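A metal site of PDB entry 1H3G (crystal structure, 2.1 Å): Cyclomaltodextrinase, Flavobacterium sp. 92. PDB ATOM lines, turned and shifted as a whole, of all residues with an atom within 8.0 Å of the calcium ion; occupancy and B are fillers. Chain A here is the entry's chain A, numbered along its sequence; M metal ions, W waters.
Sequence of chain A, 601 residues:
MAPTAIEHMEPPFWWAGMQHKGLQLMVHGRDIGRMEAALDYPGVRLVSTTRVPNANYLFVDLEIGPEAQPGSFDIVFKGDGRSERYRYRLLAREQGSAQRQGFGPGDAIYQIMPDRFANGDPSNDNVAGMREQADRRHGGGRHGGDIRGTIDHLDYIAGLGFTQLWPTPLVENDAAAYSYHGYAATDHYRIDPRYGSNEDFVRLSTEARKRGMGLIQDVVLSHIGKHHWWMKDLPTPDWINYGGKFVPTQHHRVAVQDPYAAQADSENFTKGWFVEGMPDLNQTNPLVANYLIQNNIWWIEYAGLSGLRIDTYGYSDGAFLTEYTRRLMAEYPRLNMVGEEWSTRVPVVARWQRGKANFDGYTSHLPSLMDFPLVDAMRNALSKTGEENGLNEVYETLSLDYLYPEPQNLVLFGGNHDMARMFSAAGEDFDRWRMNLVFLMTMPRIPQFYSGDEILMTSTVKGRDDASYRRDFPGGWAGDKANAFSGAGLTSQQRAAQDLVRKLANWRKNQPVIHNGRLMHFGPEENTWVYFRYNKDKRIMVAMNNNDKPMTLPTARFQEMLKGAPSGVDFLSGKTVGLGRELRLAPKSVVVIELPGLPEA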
ATOM      1  N   PRO A 114     -16.278 -13.754   1.894  1.00  0.00           N
ATOM      2  CA  PRO A 114     -17.437 -13.090   2.514  1.00  0.00           C
ATOM      3  C   PRO A 114     -18.669 -13.939   2.555  1.00  0.00           C
ATOM      4  O   PRO A 114     -19.320 -14.001   3.574  1.00  0.00           O
ATOM      5  CB  PRO A 114     -17.631 -11.868   1.643  1.00  0.00           C
ATOM      6  CG  PRO A 114     -16.329 -11.619   1.090  1.00  0.00           C
ATOM      7  CD  PRO A 114     -15.678 -12.944   0.851  1.00  0.00           C
ATOM      8  N   ASP A 115     -18.974 -14.634   1.459  1.00  0.00           N
ATOM      9  CA  ASP A 115     -20.150 -15.468   1.430  1.00  0.00           C
ATOM     10  C   ASP A 115     -20.122 -16.612   2.419  1.00  0.00           C
ATOM     11  O   ASP A 115     -21.161 -17.129   2.788  1.00  0.00           O
ATOM     12  CB  ASP A 115     -20.334 -16.068   0.051  1.00  0.00           C
ATOM     13  CG  ASP A 115     -21.629 -16.806  -0.067  1.00  0.00           C
ATOM     14  OD1 ASP A 115     -21.602 -18.044  -0.249  1.00  0.00           O
ATOM     15  OD2 ASP A 115     -22.716 -16.210   0.016  1.00  0.00           O
ATOM     16  N   ALA A 118     -19.658 -15.214   7.701  1.00  0.00           N
ATOM     17  CA  ALA A 118     -20.738 -14.979   8.607  1.00  0.00           C
ATOM     18  C   ALA A 118     -21.903 -14.283   7.908  1.00  0.00           C
ATOM     19  O   ALA A 118     -21.741 -13.264   7.243  1.00  0.00           O
ATOM     20  CB  ALA A 118     -20.259 -14.142   9.789  1.00  0.00           C
ATOM     21  N   ASN A 119     -23.092 -14.874   8.095  1.00  0.00           N
ATOM     22  CA  ASN A 119     -24.346 -14.325   7.592  1.00  0.00           C
ATOM     23  C   ASN A 119     -24.965 -13.466   8.684  1.00  0.00           C
ATOM     24  O   ASN A 119     -25.753 -13.945   9.475  1.00  0.00           O
ATOM     25  CB  ASN A 119     -25.294 -15.458   7.229  1.00  0.00           C
ATOM     26  CG  ASN A 119     -26.497 -14.986   6.429  1.00  0.00           C
ATOM     27  OD1 ASN A 119     -26.733 -13.783   6.276  1.00  0.00           O
ATOM     28  ND2 ASN A 119     -27.260 -15.939   5.903  1.00  0.00           N
ATOM     29  N   GLY A 120     -24.619 -12.195   8.709  1.00  0.00           N
ATOM     30  CA  GLY A 120     -25.124 -11.289   9.728  1.00  0.00           C
ATOM     31  C   GLY A 120     -26.492 -10.745   9.380  1.00  0.00           C
ATOM     32  O   GLY A 120     -27.155 -10.140  10.223  1.00  0.00           O
ATOM     33  N   ASP A 121     -26.912 -10.953   8.144  1.00  0.00           N
ATOM     34  CA  ASP A 121     -28.205 -10.462   7.662  1.00  0.00           C
ATOM     35  C   ASP A 121     -28.791 -11.412   6.614  1.00  0.00           C
ATOM     36  O   ASP A 121     -28.540 -11.295   5.425  1.00  0.00           O
ATOM     37  CB  ASP A 121     -27.998  -9.094   7.055  1.00  0.00           C
ATOM     38  CG  ASP A 121     -29.288  -8.417   6.650  1.00  0.00           C
ATOM     39  OD1 ASP A 121     -30.370  -9.033   6.771  1.00  0.00           O
ATOM     40  OD2 ASP A 121     -29.284  -7.256   6.190  1.00  0.00           O
ATOM     41  N   PRO A 122     -29.622 -12.346   7.063  1.00  0.00           N
ATOM     42  CA  PRO A 122     -30.281 -13.284   6.149  1.00  0.00           C
ATOM     43  C   PRO A 122     -31.180 -12.622   5.092  1.00  0.00           C
ATOM     44  O   PRO A 122     -31.434 -13.238   4.053  1.00  0.00           O
ATOM     45  CB  PRO A 122     -31.141 -14.136   7.103  1.00  0.00           C
ATOM     46  CG  PRO A 122     -30.510 -13.948   8.471  1.00  0.00           C
ATOM     47  CD  PRO A 122     -30.017 -12.546   8.466  1.00  0.00           C
ATOM     48  N   SER A 123     -31.624 -11.392   5.336  1.00  0.00           N
ATOM     49  CA  SER A 123     -32.515 -10.699   4.396  1.00  0.00           C
ATOM     50  C   SER A 123     -31.830 -10.284   3.102  1.00  0.00           C
ATOM     51  O   SER A 123     -32.490  -9.918   2.148  1.00  0.00           O
ATOM     52  CB  SER A 123     -33.157  -9.471   5.047  1.00  0.00           C
ATOM     53  OG  SER A 123     -32.182  -8.477   5.314  1.00  0.00           O
ATOM     54  N   ASN A 124     -30.499 -10.300   3.068  1.00  0.00           N
ATOM     55  CA  ASN A 124     -29.795  -9.971   1.840  1.00  0.00           C
ATOM     56  C   ASN A 124     -29.239 -11.194   1.138  1.00  0.00           C
ATOM     57  O   ASN A 124     -28.571 -11.073   0.106  1.00  0.00           O
ATOM     58  CB  ASN A 124     -28.701  -8.943   2.101  1.00  0.00           C
ATOM     59  CG  ASN A 124     -27.559  -9.495   2.957  1.00  0.00           C
ATOM     60  OD1 ASN A 124     -27.403 -10.708   3.125  1.00  0.00           O
ATOM     61  ND2 ASN A 124     -26.763  -8.592   3.489  1.00  0.00           N
ATOM     62  N   ASP A 125     -29.521 -12.385   1.681  1.00  0.00           N
ATOM     63  CA  ASP A 125     -29.053 -13.619   1.066  1.00  0.00           C
ATOM     64  C   ASP A 125     -29.568 -13.661  -0.349  1.00  0.00           C
ATOM     65  O   ASP A 125     -28.888 -14.108  -1.262  1.00  0.00           O
ATOM     66  CB  ASP A 125     -29.534 -14.849   1.837  1.00  0.00           C
ATOM     67  CG  ASP A 125     -28.937 -14.940   3.211  1.00  0.00           C
ATOM     68  OD1 ASP A 125     -28.128 -14.046   3.591  1.00  0.00           O
ATOM     69  OD2 ASP A 125     -29.216 -15.850   3.992  1.00  0.00           O
ATOM     70  N   ASN A 126     -30.795 -13.183  -0.540  1.00  0.00           N
ATOM     71  CA  ASN A 126     -31.327 -13.049  -1.877  1.00  0.00           C
ATOM     72  C   ASN A 126     -31.723 -11.600  -2.101  1.00  0.00           C
ATOM     73  O   ASN A 126     -32.156 -10.916  -1.182  1.00  0.00           O
ATOM     74  CB  ASN A 126     -32.522 -13.965  -2.094  1.00  0.00           C
ATOM     75  CG  ASN A 126     -32.123 -15.413  -2.255  1.00  0.00           C
ATOM     76  OD1 ASN A 126     -31.264 -15.761  -3.092  1.00  0.00           O
ATOM     77  ND2 ASN A 126     -32.709 -16.274  -1.446  1.00  0.00           N
ATOM     78  N   ALA A 134     -29.765 -17.878  -3.420  1.00  0.00           N
ATOM     79  CA  ALA A 134     -28.933 -18.506  -2.421  1.00  0.00           C
ATOM     80  C   ALA A 134     -29.277 -19.973  -2.249  1.00  0.00           C
ATOM     81  O   ALA A 134     -30.415 -20.377  -2.417  1.00  0.00           O
ATOM     82  CB  ALA A 134     -29.114 -17.786  -1.090  1.00  0.00           C
ATOM     83  N   ARG A 142     -24.548 -19.677  -3.256  1.00  0.00           N
ATOM     84  CA  ARG A 142     -24.411 -18.579  -2.335  1.00  0.00           C
ATOM     85  C   ARG A 142     -24.939 -19.025  -0.985  1.00  0.00           C
ATOM     86  O   ARG A 142     -26.059 -19.497  -0.864  1.00  0.00           O
ATOM     87  CB  ARG A 142     -25.193 -17.384  -2.802  1.00  0.00           C
ATOM     88  CG  ARG A 142     -24.704 -16.742  -4.073  1.00  0.00           C
ATOM     89  CD  ARG A 142     -25.233 -15.333  -4.237  1.00  0.00           C
ATOM     90  NE  ARG A 142     -24.627 -14.434  -3.267  1.00  0.00           N
ATOM     91  CZ  ARG A 142     -23.562 -13.705  -3.503  1.00  0.00           C
ATOM     92  NH1 ARG A 142     -22.969 -13.756  -4.705  1.00  0.00           N
ATOM     93  NH2 ARG A 142     -23.058 -12.919  -2.555  1.00  0.00           N
ATOM     94  N   HIS A 143     -24.127 -18.827   0.046  1.00  0.00           N
ATOM     95  CA  HIS A 143     -24.482 -19.264   1.370  1.00  0.00           C
ATOM     96  C   HIS A 143     -25.035 -18.171   2.242  1.00  0.00           C
ATOM     97  O   HIS A 143     -25.661 -18.463   3.250  1.00  0.00           O
ATOM     98  CB  HIS A 143     -23.286 -19.918   2.030  1.00  0.00           C
ATOM     99  CG  HIS A 143     -22.947 -21.242   1.446  1.00  0.00           C
ATOM    100  ND1 HIS A 143     -22.136 -22.153   2.081  1.00  0.00           N
ATOM    101  CD2 HIS A 143     -23.343 -21.831   0.291  1.00  0.00           C
ATOM    102  CE1 HIS A 143     -22.047 -23.248   1.338  1.00  0.00           C
ATOM    103  NE2 HIS A 143     -22.754 -23.067   0.240  1.00  0.00           N
ATOM    104  N   GLY A 144     -24.791 -16.920   1.856  1.00  0.00           N
ATOM    105  CA  GLY A 144     -25.390 -15.793   2.548  1.00  0.00           C
ATOM    106  C   GLY A 144     -24.468 -15.002   3.424  1.00  0.00           C
ATOM    107  O   GLY A 144     -24.924 -14.089   4.113  1.00  0.00           O
ATOM    108  N   GLY A 145     -23.182 -15.313   3.411  1.00  0.00           N
ATOM    109  CA  GLY A 145     -22.250 -14.554   4.203  1.00  0.00           C
ATOM    110  C   GLY A 145     -22.289 -13.121   3.719  1.00  0.00           C
ATOM    111  O   GLY A 145     -22.509 -12.874   2.530  1.00  0.00           O
ATOM    112  N   ASP A 146     -22.062 -12.171   4.616  1.00  0.00           N
ATOM    113  CA  ASP A 146     -22.159 -10.773   4.240  1.00  0.00           C
ATOM    114  C   ASP A 146     -21.294  -9.887   5.126  1.00  0.00           C
ATOM    115  O   ASP A 146     -20.668 -10.340   6.069  1.00  0.00           O
ATOM    116  CB  ASP A 146     -23.626 -10.335   4.283  1.00  0.00           C
ATOM    117  CG  ASP A 146     -24.289 -10.658   5.608  1.00  0.00           C
ATOM    118  OD1 ASP A 146     -25.439 -11.157   5.629  1.00  0.00           O
ATOM    119  OD2 ASP A 146     -23.712 -10.468   6.678  1.00  0.00           O
ATOM    120  N   ILE A 147     -21.257  -8.600   4.783  1.00  0.00           N
ATOM    121  CA  ILE A 147     -20.451  -7.611   5.480  1.00  0.00           C
ATOM    122  C   ILE A 147     -20.929  -7.446   6.904  1.00  0.00           C
ATOM    123  O   ILE A 147     -20.131  -7.363   7.818  1.00  0.00           O
ATOM    124  CB  ILE A 147     -20.511  -6.280   4.730  1.00  0.00           C
ATOM    125  CG1 ILE A 147     -19.770  -6.415   3.388  1.00  0.00           C
ATOM    126  CG2 ILE A 147     -19.892  -5.176   5.534  1.00  0.00           C
ATOM    127  CD1 ILE A 147     -19.929  -5.211   2.485  1.00  0.00           C
ATOM    128  N   ARG A 148     -22.237  -7.414   7.112  1.00  0.00           N
ATOM    129  CA  ARG A 148     -22.746  -7.310   8.466  1.00  0.00           C
ATOM    130  C   ARG A 148     -22.151  -8.464   9.308  1.00  0.00           C
ATOM    131  O   ARG A 148     -21.659  -8.266  10.420  1.00  0.00           O
ATOM    132  CB  ARG A 148     -24.287  -7.287   8.476  1.00  0.00           C
ATOM    133  CG  ARG A 148     -24.936  -7.277   9.881  1.00  0.00           C
ATOM    134  CD  ARG A 148     -24.232  -6.423  10.904  1.00  0.00           C
ATOM    135  NE  ARG A 148     -24.031  -5.041  10.470  1.00  0.00           N
ATOM    136  CZ  ARG A 148     -23.198  -4.183  11.059  1.00  0.00           C
ATOM    137  NH1 ARG A 148     -22.497  -4.550  12.122  1.00  0.00           N
ATOM    138  NH2 ARG A 148     -23.066  -2.956  10.596  1.00  0.00           N
ATOM    139  N   GLY A 149     -22.164  -9.676   8.762  1.00  0.00           N
ATOM    140  CA  GLY A 149     -21.601 -10.799   9.489  1.00  0.00           C
ATOM    141  C   GLY A 149     -20.132 -10.602   9.809  1.00  0.00           C
ATOM    142  O   GLY A 149     -19.690 -10.905  10.911  1.00  0.00           O
ATOM    143  N   PRO A 193     -24.958  -6.556  -3.849  1.00  0.00           N
ATOM    144  CA  PRO A 193     -26.026  -6.237  -2.901  1.00  0.00           C
ATOM    145  C   PRO A 193     -26.224  -7.333  -1.897  1.00  0.00           C
ATOM    146  O   PRO A 193     -26.670  -7.057  -0.800  1.00  0.00           O
ATOM    147  CB  PRO A 193     -27.262  -6.102  -3.793  1.00  0.00           C
ATOM    148  CG  PRO A 193     -26.748  -5.938  -5.154  1.00  0.00           C
ATOM    149  CD  PRO A 193     -25.444  -6.612  -5.246  1.00  0.00           C
ATOM    150  N   ARG A 194     -25.870  -8.565  -2.254  1.00  0.00           N
ATOM    151  CA  ARG A 194     -25.997  -9.693  -1.338  1.00  0.00           C
ATOM    152  C   ARG A 194     -25.053  -9.578  -0.168  1.00  0.00           C
ATOM    153  O   ARG A 194     -25.294 -10.156   0.883  1.00  0.00           O
ATOM    154  CB  ARG A 194     -25.755 -11.010  -2.079  1.00  0.00           C
ATOM    155  CG  ARG A 194     -26.996 -11.654  -2.632  1.00  0.00           C
ATOM    156  CD  ARG A 194     -27.212 -11.697  -4.129  1.00  0.00           C
ATOM    157  NE  ARG A 194     -26.062 -11.612  -5.008  1.00  0.00           N
ATOM    158  CZ  ARG A 194     -25.912 -12.308  -6.130  1.00  0.00           C
ATOM    159  NH1 ARG A 194     -26.781 -13.242  -6.495  1.00  0.00           N
ATOM    160  NH2 ARG A 194     -24.861 -12.091  -6.887  1.00  0.00           N
ATOM    161  N   TYR A 195     -23.975  -8.810  -0.340  1.00  0.00           N
ATOM    162  CA  TYR A 195     -23.019  -8.592   0.752  1.00  0.00           C
ATOM    163  C   TYR A 195     -23.341  -7.342   1.523  1.00  0.00           C
ATOM    164  O   TYR A 195     -23.021  -7.232   2.713  1.00  0.00           O
ATOM    165  CB  TYR A 195     -21.612  -8.422   0.200  1.00  0.00           C
ATOM    166  CG  TYR A 195     -21.066  -9.675  -0.381  1.00  0.00           C
ATOM    167  CD1 TYR A 195     -21.300 -10.901   0.217  1.00  0.00           C
ATOM    168  CD2 TYR A 195     -20.330  -9.640  -1.550  1.00  0.00           C
ATOM    169  CE1 TYR A 195     -20.793 -12.072  -0.317  1.00  0.00           C
ATOM    170  CE2 TYR A 195     -19.831 -10.806  -2.107  1.00  0.00           C
ATOM    171  CZ  TYR A 195     -20.058 -12.007  -1.493  1.00  0.00           C
ATOM    172  OH  TYR A 195     -19.570 -13.155  -2.056  1.00  0.00           O
ATOM    173  N   GLY A 196     -23.938  -6.385   0.836  1.00  0.00           N
ATOM    174  CA  GLY A 196     -24.238  -5.122   1.461  1.00  0.00           C
ATOM    175  C   GLY A 196     -24.137  -4.036   0.429  1.00  0.00           C
ATOM    176  O   GLY A 196     -24.157  -4.301  -0.761  1.00  0.00           O
ATOM    177  N   TRP A 477     -23.566 -18.803  10.862  1.00  0.00           N
ATOM    178  CA  TRP A 477     -24.999 -18.800  10.587  1.00  0.00           C
ATOM    179  C   TRP A 477     -25.798 -19.105  11.841  1.00  0.00           C
ATOM    180  O   TRP A 477     -25.392 -19.917  12.668  1.00  0.00           O
ATOM    181  CB  TRP A 477     -25.358 -19.838   9.533  1.00  0.00           C
ATOM    182  CG  TRP A 477     -25.121 -19.360   8.145  1.00  0.00           C
ATOM    183  CD1 TRP A 477     -26.054 -19.131   7.177  1.00  0.00           C
ATOM    184  CD2 TRP A 477     -23.857 -19.082   7.549  1.00  0.00           C
ATOM    185  NE1 TRP A 477     -25.440 -18.726   6.012  1.00  0.00           N
ATOM    186  CE2 TRP A 477     -24.084 -18.676   6.224  1.00  0.00           C
ATOM    187  CE3 TRP A 477     -22.538 -19.132   8.011  1.00  0.00           C
ATOM    188  CZ2 TRP A 477     -23.051 -18.323   5.356  1.00  0.00           C
ATOM    189  CZ3 TRP A 477     -21.516 -18.777   7.152  1.00  0.00           C
ATOM    190  CH2 TRP A 477     -21.775 -18.377   5.846  1.00  0.00           C
HETATM  191 CA    CA M   1     -26.711 -12.495   4.299  1.00  0.00          CA
HETATM  192  O   HOH W   1     -25.891 -12.354   1.999  1.00  0.00           O
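The side-chain carboxylate (OD2) of Asp 146 is in hydrogen-bond range of the backbone NH (N) of Gly 120 (2.8 Å).
N of Asp 146 sits at hydrogen-bond distance from O of Ala 118 (2.9 Å).
ND2 of Asn 119 sits close to NE1 of Trp 477 (3.3 Å).
O of Arg 194 sits close to ND2 of Asn 124.
OD1 of Asp 121 is in hydrogen-bond range of N of Ser 123, at 3.0 Å.
OD2 of Asp 146 lies within hydrogen-bond range of N of Gly 149.
The backbone NH (N) of Asp 146 sits at hydrogen-bond distance from the backbone carbonyl oxygen (O) of Pro 114 (3.5 Å).
The side-chain carboxylate (OD2) of Asp 146 sits close to the backbone NH (N) of Arg 148 (3.4 Å).
Of the 25 residues printed, 6 come within 4 Å of the calcium ion.
The calcium ion is bound by OD1 of Asp 125 (2.2 Å), OD1 of Asn 124 (2.2 Å), OD1 of Asp 146 (2.3 Å), OD1 of Asn 119 (2.4 Å), O of Gly 144 (2.4 Å), water W1 (2.4 Å) and O of Asp 121 (2.5 Å).
The calcium ion has seven donor atoms within binding distance.
Water W1 bridges O of Arg 194 (2.5 Å) and O of Gly 145 (3.5 Å).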
